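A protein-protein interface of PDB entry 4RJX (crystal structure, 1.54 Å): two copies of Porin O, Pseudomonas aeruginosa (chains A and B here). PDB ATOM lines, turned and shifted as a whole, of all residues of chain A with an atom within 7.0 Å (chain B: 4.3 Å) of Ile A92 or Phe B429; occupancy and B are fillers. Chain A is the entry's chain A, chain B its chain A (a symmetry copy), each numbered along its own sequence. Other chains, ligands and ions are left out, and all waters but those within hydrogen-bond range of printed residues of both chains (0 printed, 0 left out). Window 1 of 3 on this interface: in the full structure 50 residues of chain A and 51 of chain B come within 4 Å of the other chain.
The backbone NH (N) of Ala A84 sits at hydrogen-bond distance from the side-chain hydroxyl (OH) of Tyr B427, at 3.2 Å. OH of Tyr A90 lies within hydrogen-bond range of O of Gly B31.
O of Leu A80 lies close to NE2 of Gln A91 (3.5 Å). O of Phe B429 sits at hydrogen-bond distance from N of Gly B48 (3.0 Å). The backbone carbonyl oxygen of Gly A82 is in hydrogen-bond range of the backbone NH of Tyr A90 (3.0 Å). The backbone NH (N) of Ile A78 is in hydrogen-bond range of the backbone carbonyl oxygen (O) of Phe A94 (2.9 Å). The backbone NH of Gly B32 lies within hydrogen-bond range of the chain-end carboxylate of Phe B429. N of Ile A92 sits at hydrogen-bond distance from O of Leu A80 (2.7 Å).
Among the printed residues, merely in contact across the chains: Tyr A90 with Phe B429 (3.2 Å), Phe A44 with Gly B31 (3.3 Å), Phe A44 with Gly B32 (3.3 Å), Tyr A90 with Tyr B427 (3.4 Å), Leu A80 with Leu B46 (3.5 Å), Ile A92 with Leu B96 (3.6 Å), Phe A94 with Leu B96 (3.6 Å), Phe A108 with Leu B96 (3.6 Å), Phe A44 with Leu B46 (3.6 Å), Ile A92 with Phe B429 (3.8 Å) and Gly A82 with Tyr B427 (3.96 Å).
Of the printed residues of chain B, Ile A92 touches Leu B96 (3.6 Å) and Phe B429 (3.8 Å). Phe B429 touches just these residues of chain A: Tyr A90 (3.2 Å) and Ile A92 (3.8 Å). Printed residues of chain B within 4 Å of Phe A44: Gly B31 (3.3 Å), Gly B32 (3.3 Å) and Leu B46 (3.6 Å). Printed residues of chain A within 4 Å of Leu B46: Phe A44 (3.6 Å) and Leu A80 (3.5 Å). Ala A111 touches none of the printed residues of chain B. Asn A93 touches none of the printed residues of chain B. The nearest printed residue of chain B that does not touch Ile A92 is Arg B49 (5.8 Å).
Hydrophobic or aromatic side chains of chain A that line the printed part of chain B: Phe A44, Leu A80, Ala A84, Tyr A90, Ile A92, Phe A94 and Phe A108. Of the 10 printed residues of chain B, 6 touch a printed residue of chain A. Along chain B the printed residues that touch a printed residue of chain A span positions 31 to 429. Among the printed residues, 13 pairs touch across the chains. Among the printed residues, no Asp or Glu carboxylate lies within 4 Å of a Lys or Arg side-chain nitrogen of the other chain.
No position is printed for both chains.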
ATOM      1  N   PHE A  44     -25.052  -0.555 -39.701  1.00  0.00           N
ATOM      2  CA  PHE A  44     -25.519  -0.942 -38.380  1.00  0.00           C
ATOM      3  C   PHE A  44     -25.355  -2.449 -38.201  1.00  0.00           C
ATOM      4  O   PHE A  44     -25.636  -3.222 -39.120  1.00  0.00           O
ATOM      5  CB  PHE A  44     -26.986  -0.539 -38.171  1.00  0.00           C
ATOM      6  CG  PHE A  44     -27.576  -1.063 -36.881  1.00  0.00           C
ATOM      7  CD1 PHE A  44     -27.101  -0.613 -35.661  1.00  0.00           C
ATOM      8  CD2 PHE A  44     -28.582  -2.015 -36.898  1.00  0.00           C
ATOM      9  CE1 PHE A  44     -27.615  -1.098 -34.467  1.00  0.00           C
ATOM     10  CE2 PHE A  44     -29.115  -2.500 -35.698  1.00  0.00           C
ATOM     11  CZ  PHE A  44     -28.626  -2.039 -34.485  1.00  0.00           C
ATOM     12  N   ILE A  78     -24.967  -7.896 -25.300  1.00  0.00           N
ATOM     13  CA  ILE A  78     -25.701  -7.385 -26.457  1.00  0.00           C
ATOM     14  C   ILE A  78     -24.798  -6.333 -27.070  1.00  0.00           C
ATOM     15  O   ILE A  78     -24.243  -5.502 -26.346  1.00  0.00           O
ATOM     16  CB  ILE A  78     -27.066  -6.768 -26.067  1.00  0.00           C
ATOM     17  CG1 ILE A  78     -27.929  -7.783 -25.299  1.00  0.00           C
ATOM     18  CG2 ILE A  78     -27.786  -6.217 -27.317  1.00  0.00           C
ATOM     19  CD1 ILE A  78     -28.110  -9.116 -26.025  1.00  0.00           C
ATOM     20  N   GLU A  79     -24.631  -6.385 -28.395  1.00  0.00           N
ATOM     21  CA  GLU A  79     -23.584  -5.612 -29.065  1.00  0.00           C
ATOM     22  C   GLU A  79     -24.187  -4.783 -30.194  1.00  0.00           C
ATOM     23  O   GLU A  79     -24.733  -5.333 -31.160  1.00  0.00           O
ATOM     24  CB  GLU A  79     -22.481  -6.549 -29.595  1.00  0.00           C
ATOM     25  CG  GLU A  79     -21.810  -7.365 -28.501  1.00  0.00           C
ATOM     26  CD  GLU A  79     -21.015  -8.545 -29.015  1.00  0.00           C
ATOM     27  OE1 GLU A  79     -20.540  -8.497 -30.168  1.00  0.00           O
ATOM     28  OE2 GLU A  79     -20.880  -9.530 -28.257  1.00  0.00           O
ATOM     29  N   LEU A  80     -24.119  -3.461 -30.056  1.00  0.00           N
ATOM     30  CA  LEU A  80     -24.639  -2.553 -31.081  1.00  0.00           C
ATOM     31  C   LEU A  80     -23.510  -1.707 -31.615  1.00  0.00           C
ATOM     32  O   LEU A  80     -22.807  -1.058 -30.853  1.00  0.00           O
ATOM     33  CB  LEU A  80     -25.728  -1.626 -30.524  1.00  0.00           C
ATOM     34  CG  LEU A  80     -27.134  -2.134 -30.224  1.00  0.00           C
ATOM     35  CD1 LEU A  80     -27.207  -2.833 -28.887  1.00  0.00           C
ATOM     36  CD2 LEU A  80     -28.102  -0.950 -30.266  1.00  0.00           C
ATOM     37  N   GLY A  81     -23.341  -1.686 -32.929  1.00  0.00           N
ATOM     38  CA  GLY A  81     -22.261  -0.896 -33.477  1.00  0.00           C
ATOM     39  C   GLY A  81     -22.676  -0.399 -34.840  1.00  0.00           C
ATOM     40  O   GLY A  81     -23.583  -0.950 -35.460  1.00  0.00           O
ATOM     41  N   GLY A  82     -22.025   0.650 -35.302  1.00  0.00           N
ATOM     42  CA  GLY A  82     -22.398   1.197 -36.594  1.00  0.00           C
ATOM     43  C   GLY A  82     -21.440   2.249 -37.094  1.00  0.00           C
ATOM     44  O   GLY A  82     -20.484   2.613 -36.414  1.00  0.00           O
ATOM     45  N   ALA A  84     -21.358   6.060 -39.415  1.00  0.00           N
ATOM     46  CA  ALA A  84     -22.098   7.178 -39.997  1.00  0.00           C
ATOM     47  C   ALA A  84     -21.117   8.114 -40.677  1.00  0.00           C
ATOM     48  O   ALA A  84     -20.029   8.358 -40.160  1.00  0.00           O
ATOM     49  CB  ALA A  84     -22.906   7.916 -38.939  1.00  0.00           C
ATOM     50  N   TYR A  90     -19.304   3.779 -33.903  1.00  0.00           N
ATOM     51  CA  TYR A  90     -19.568   3.571 -32.475  1.00  0.00           C
ATOM     52  C   TYR A  90     -19.682   2.090 -32.192  1.00  0.00           C
ATOM     53  O   TYR A  90     -20.007   1.298 -33.081  1.00  0.00           O
ATOM     54  CB  TYR A  90     -20.849   4.286 -32.027  1.00  0.00           C
ATOM     55  CG  TYR A  90     -22.128   3.611 -32.494  1.00  0.00           C
ATOM     56  CD1 TYR A  90     -22.635   3.844 -33.768  1.00  0.00           C
ATOM     57  CD2 TYR A  90     -22.820   2.731 -31.664  1.00  0.00           C
ATOM     58  CE1 TYR A  90     -23.800   3.233 -34.204  1.00  0.00           C
ATOM     59  CE2 TYR A  90     -23.988   2.113 -32.093  1.00  0.00           C
ATOM     60  CZ  TYR A  90     -24.470   2.361 -33.365  1.00  0.00           C
ATOM     61  OH  TYR A  90     -25.626   1.735 -33.789  1.00  0.00           O
ATOM     62  N   GLN A  91     -19.406   1.717 -30.947  1.00  0.00           N
ATOM     63  CA  GLN A  91     -19.597   0.340 -30.506  1.00  0.00           C
ATOM     64  C   GLN A  91     -20.027   0.342 -29.052  1.00  0.00           C
ATOM     65  O   GLN A  91     -19.320   0.866 -28.185  1.00  0.00           O
ATOM     66  CB  GLN A  91     -18.321  -0.484 -30.680  1.00  0.00           C
ATOM     67  CG  GLN A  91     -18.524  -1.976 -30.417  1.00  0.00           C
ATOM     68  CD  GLN A  91     -19.359  -2.635 -31.500  1.00  0.00           C
ATOM     69  OE1 GLN A  91     -19.165  -2.379 -32.699  1.00  0.00           O
ATOM     70  NE2 GLN A  91     -20.298  -3.487 -31.090  1.00  0.00           N
ATOM     71  N   ILE A  92     -21.187  -0.254 -28.791  1.00  0.00           N
ATOM     72  CA  ILE A  92     -21.743  -0.325 -27.435  1.00  0.00           C
ATOM     73  C   ILE A  92     -22.064  -1.772 -27.112  1.00  0.00           C
ATOM     74  O   ILE A  92     -22.994  -2.355 -27.689  1.00  0.00           O
ATOM     75  CB  ILE A  92     -23.028   0.522 -27.304  1.00  0.00           C
ATOM     76  CG1 ILE A  92     -22.758   1.981 -27.669  1.00  0.00           C
ATOM     77  CG2 ILE A  92     -23.616   0.419 -25.880  1.00  0.00           C
ATOM     78  CD1 ILE A  92     -24.038   2.754 -27.967  1.00  0.00           C
ATOM     79  N   ASN A  93     -21.292  -2.347 -26.193  1.00  0.00           N
ATOM     80  CA  ASN A  93     -21.457  -3.738 -25.795  1.00  0.00           C
ATOM     81  C   ASN A  93     -21.812  -3.760 -24.332  1.00  0.00           C
ATOM     82  O   ASN A  93     -20.982  -3.378 -23.497  1.00  0.00           O
ATOM     83  CB  ASN A  93     -20.177  -4.555 -26.018  1.00  0.00           C
ATOM     84  CG  ASN A  93     -19.750  -4.608 -27.474  1.00  0.00           C
ATOM     85  OD1 ASN A  93     -20.531  -4.330 -28.380  1.00  0.00           O
ATOM     86  ND2 ASN A  93     -18.492  -4.976 -27.699  1.00  0.00           N
ATOM     87  N   PHE A  94     -23.031  -4.172 -24.004  1.00  0.00           N
ATOM     88  CA  PHE A  94     -23.408  -4.197 -22.590  1.00  0.00           C
ATOM     89  C   PHE A  94     -23.668  -5.632 -22.133  1.00  0.00           C
ATOM     90  O   PHE A  94     -24.165  -6.470 -22.887  1.00  0.00           O
ATOM     91  CB  PHE A  94     -24.606  -3.262 -22.293  1.00  0.00           C
ATOM     92  CG  PHE A  94     -25.878  -3.514 -23.106  1.00  0.00           C
ATOM     93  CD1 PHE A  94     -26.024  -2.994 -24.386  1.00  0.00           C
ATOM     94  CD2 PHE A  94     -26.950  -4.190 -22.542  1.00  0.00           C
ATOM     95  CE1 PHE A  94     -27.216  -3.177 -25.096  1.00  0.00           C
ATOM     96  CE2 PHE A  94     -28.144  -4.385 -23.252  1.00  0.00           C
ATOM     97  CZ  PHE A  94     -28.270  -3.881 -24.526  1.00  0.00           C
ATOM     98  N   PHE A 108     -20.742  -1.981 -18.987  1.00  0.00           N
ATOM     99  CA  PHE A 108     -20.117  -1.865 -20.296  1.00  0.00           C
ATOM    100  C   PHE A 108     -18.924  -2.792 -20.472  1.00  0.00           C
ATOM    101  O   PHE A 108     -17.971  -2.732 -19.696  1.00  0.00           O
ATOM    102  CB  PHE A 108     -19.635  -0.425 -20.534  1.00  0.00           C
ATOM    103  CG  PHE A 108     -20.732   0.595 -20.585  1.00  0.00           C
ATOM    104  CD1 PHE A 108     -21.585   0.652 -21.686  1.00  0.00           C
ATOM    105  CD2 PHE A 108     -20.884   1.532 -19.573  1.00  0.00           C
ATOM    106  CE1 PHE A 108     -22.605   1.597 -21.750  1.00  0.00           C
ATOM    107  CE2 PHE A 108     -21.895   2.490 -19.632  1.00  0.00           C
ATOM    108  CZ  PHE A 108     -22.755   2.521 -20.732  1.00  0.00           C
ATOM    109  N   ASP A 109     -18.966  -3.629 -21.504  1.00  0.00           N
ATOM    110  CA  ASP A 109     -17.730  -4.189 -22.040  1.00  0.00           C
ATOM    111  C   ASP A 109     -17.032  -3.089 -22.851  1.00  0.00           C
ATOM    112  O   ASP A 109     -15.809  -2.932 -22.802  1.00  0.00           O
ATOM    113  CB  ASP A 109     -18.019  -5.419 -22.906  1.00  0.00           C
ATOM    114  CG  ASP A 109     -16.871  -5.765 -23.843  1.00  0.00           C
ATOM    115  OD1 ASP A 109     -15.883  -6.369 -23.377  1.00  0.00           O
ATOM    116  OD2 ASP A 109     -16.970  -5.450 -25.049  1.00  0.00           O
ATOM    117  N   GLU A 110     -17.831  -2.303 -23.570  1.00  0.00           N
ATOM    118  CA  GLU A 110     -17.314  -1.227 -24.421  1.00  0.00           C
ATOM    119  C   GLU A 110     -18.406  -0.198 -24.667  1.00  0.00           C
ATOM    120  O   GLU A 110     -19.572  -0.552 -24.855  1.00  0.00           O
ATOM    121  CB  GLU A 110     -16.803  -1.768 -25.768  1.00  0.00           C
ATOM    122  CG  GLU A 110     -16.138  -0.693 -26.628  1.00  0.00           C
ATOM    123  CD  GLU A 110     -15.496  -1.257 -27.889  1.00  0.00           C
ATOM    124  OE1 GLU A 110     -15.521  -2.493 -28.080  1.00  0.00           O
ATOM    125  OE2 GLU A 110     -14.972  -0.465 -28.702  1.00  0.00           O
ATOM    126  N   ALA A 111     -18.029   1.074 -24.639  1.00  0.00           N
ATOM    127  CA  ALA A 111     -18.881   2.138 -25.157  1.00  0.00           C
ATOM    128  C   ALA A 111     -17.936   3.166 -25.760  1.00  0.00           C
ATOM    129  O   ALA A 111     -17.356   3.985 -25.060  1.00  0.00           O
ATOM    130  CB  ALA A 111     -19.775   2.734 -24.060  1.00  0.00           C
ATOM    131  N   SER A 112     -17.736   3.069 -27.072  1.00  0.00           N
ATOM    132  CA  SER A 112     -16.678   3.848 -27.713  1.00  0.00           C
ATOM    133  C   SER A 112     -17.139   4.519 -28.992  1.00  0.00           C
ATOM    134  O   SER A 112     -18.113   4.089 -29.610  1.00  0.00           O
ATOM    135  CB  SER A 112     -15.472   2.963 -28.039  1.00  0.00           C
ATOM    136  OG  SER A 112     -15.788   1.984 -29.025  1.00  0.00           O
ATOM    137  N   GLY B  31     -26.766   4.669 -39.126  1.00  0.00           N
ATOM    138  CA  GLY B  31     -26.002   4.204 -37.985  1.00  0.00           C
ATOM    139  C   GLY B  31     -26.852   3.344 -37.074  1.00  0.00           C
ATOM    140  O   GLY B  31     -26.318   2.513 -36.350  1.00  0.00           O
ATOM    141  N   GLY B  32     -28.167   3.568 -37.102  1.00  0.00           N
ATOM    142  CA  GLY B  32     -29.124   2.695 -36.440  1.00  0.00           C
ATOM    143  C   GLY B  32     -29.970   1.980 -37.476  1.00  0.00           C
ATOM    144  O   GLY B  32     -29.477   1.623 -38.549  1.00  0.00           O
ATOM    145  N   LEU B  46     -34.704   1.545 -34.200  1.00  0.00           N
ATOM    146  CA  LEU B  46     -33.699   1.319 -33.171  1.00  0.00           C
ATOM    147  C   LEU B  46     -32.659   2.424 -33.283  1.00  0.00           C
ATOM    148  O   LEU B  46     -32.062   2.626 -34.346  1.00  0.00           O
ATOM    149  CB  LEU B  46     -33.053  -0.068 -33.312  1.00  0.00           C
ATOM    150  CG  LEU B  46     -32.026  -0.512 -32.262  1.00  0.00           C
ATOM    151  CD1 LEU B  46     -31.856  -2.029 -32.275  1.00  0.00           C
ATOM    152  CD2 LEU B  46     -30.663   0.173 -32.440  1.00  0.00           C
ATOM    153  N   GLY B  47     -32.451   3.148 -32.190  1.00  0.00           N
ATOM    154  CA  GLY B  47     -31.478   4.223 -32.173  1.00  0.00           C
ATOM    155  C   GLY B  47     -30.872   4.361 -30.801  1.00  0.00           C
ATOM    156  O   GLY B  47     -30.938   3.444 -29.990  1.00  0.00           O
ATOM    157  N   GLY B  48     -30.251   5.506 -30.554  1.00  0.00           N
ATOM    158  CA  GLY B  48     -29.673   5.761 -29.249  1.00  0.00           C
ATOM    159  C   GLY B  48     -28.841   7.021 -29.215  1.00  0.00           C
ATOM    160  O   GLY B  48     -28.761   7.769 -30.189  1.00  0.00           O
ATOM    161  N   ARG B  49     -28.223   7.270 -28.068  1.00  0.00           N
ATOM    162  CA  ARG B  49     -27.343   8.422 -27.952  1.00  0.00           C
ATOM    163  C   ARG B  49     -26.260   8.141 -26.926  1.00  0.00           C
ATOM    164  O   ARG B  49     -26.521   7.582 -25.857  1.00  0.00           O
ATOM    165  CB  ARG B  49     -28.138   9.684 -27.577  1.00  0.00           C
ATOM    166  CG  ARG B  49     -28.667   9.702 -26.140  1.00  0.00           C
ATOM    167  CD  ARG B  49     -29.761  10.748 -25.953  1.00  0.00           C
ATOM    168  NE  ARG B  49     -31.002  10.355 -26.629  1.00  0.00           N
ATOM    169  CZ  ARG B  49     -32.156  11.010 -26.525  1.00  0.00           C
ATOM    170  NH1 ARG B  49     -33.234  10.556 -27.139  1.00  0.00           N
ATOM    171  NH2 ARG B  49     -32.232  12.117 -25.790  1.00  0.00           N
ATOM    172  N   LEU B  96     -28.029   2.995 -20.332  1.00  0.00           N
ATOM    173  CA  LEU B  96     -26.975   2.074 -19.911  1.00  0.00           C
ATOM    174  C   LEU B  96     -25.985   2.707 -18.927  1.00  0.00           C
ATOM    175  O   LEU B  96     -25.276   1.995 -18.224  1.00  0.00           O
ATOM    176  CB  LEU B  96     -26.213   1.558 -21.135  1.00  0.00           C
ATOM    177  CG  LEU B  96     -27.017   0.720 -22.136  1.00  0.00           C
ATOM    178  CD1 LEU B  96     -26.140   0.442 -23.356  1.00  0.00           C
ATOM    179  CD2 LEU B  96     -27.490  -0.585 -21.516  1.00  0.00           C
ATOM    180  N   TYR B 427     -22.552  11.055 -29.844  1.00  0.00           N
ATOM    181  CA  TYR B 427     -22.854  10.287 -31.055  1.00  0.00           C
ATOM    182  C   TYR B 427     -24.321   9.871 -30.980  1.00  0.00           C
ATOM    183  O   TYR B 427     -24.743   9.230 -30.010  1.00  0.00           O
ATOM    184  CB  TYR B 427     -21.925   9.061 -31.162  1.00  0.00           C
ATOM    185  CG  TYR B 427     -21.856   8.361 -32.513  1.00  0.00           C
ATOM    186  CD1 TYR B 427     -22.994   7.854 -33.123  1.00  0.00           C
ATOM    187  CD2 TYR B 427     -20.636   8.184 -33.155  1.00  0.00           C
ATOM    188  CE1 TYR B 427     -22.925   7.206 -34.358  1.00  0.00           C
ATOM    189  CE2 TYR B 427     -20.546   7.531 -34.383  1.00  0.00           C
ATOM    190  CZ  TYR B 427     -21.699   7.047 -34.978  1.00  0.00           C
ATOM    191  OH  TYR B 427     -21.629   6.394 -36.194  1.00  0.00           O
ATOM    192  N   VAL B 428     -25.089  10.242 -31.998  1.00  0.00           N
ATOM    193  CA  VAL B 428     -26.512   9.917 -32.077  1.00  0.00           C
ATOM    194  C   VAL B 428     -26.734   8.986 -33.258  1.00  0.00           C
ATOM    195  O   VAL B 428     -26.170   9.199 -34.333  1.00  0.00           O
ATOM    196  CB  VAL B 428     -27.366  11.189 -32.236  1.00  0.00           C
ATOM    197  CG1 VAL B 428     -28.824  10.842 -32.579  1.00  0.00           C
ATOM    198  CG2 VAL B 428     -27.246  12.077 -30.987  1.00  0.00           C
ATOM    199  N   PHE B 429     -27.522   7.937 -33.054  1.00  0.00           N
ATOM    200  CA  PHE B 429     -27.786   6.975 -34.127  1.00  0.00           C
ATOM    201  C   PHE B 429     -29.243   6.523 -34.102  1.00  0.00           C
ATOM    202  O   PHE B 429     -29.992   6.895 -33.193  1.00  0.00           O
ATOM    203  CB  PHE B 429     -26.835   5.768 -34.030  1.00  0.00           C
ATOM    204  CG  PHE B 429     -26.908   5.021 -32.727  1.00  0.00           C
ATOM    205  CD1 PHE B 429     -26.151   5.424 -31.635  1.00  0.00           C
ATOM    206  CD2 PHE B 429     -27.715   3.897 -32.603  1.00  0.00           C
ATOM    207  CE1 PHE B 429     -26.208   4.727 -30.438  1.00  0.00           C
ATOM    208  CE2 PHE B 429     -27.775   3.196 -31.418  1.00  0.00           C
ATOM    209  CZ  PHE B 429     -27.024   3.610 -30.332  1.00  0.00           C
ATOM    210  OXT PHE B 429     -29.699   5.811 -35.014  1.00  0.00           O
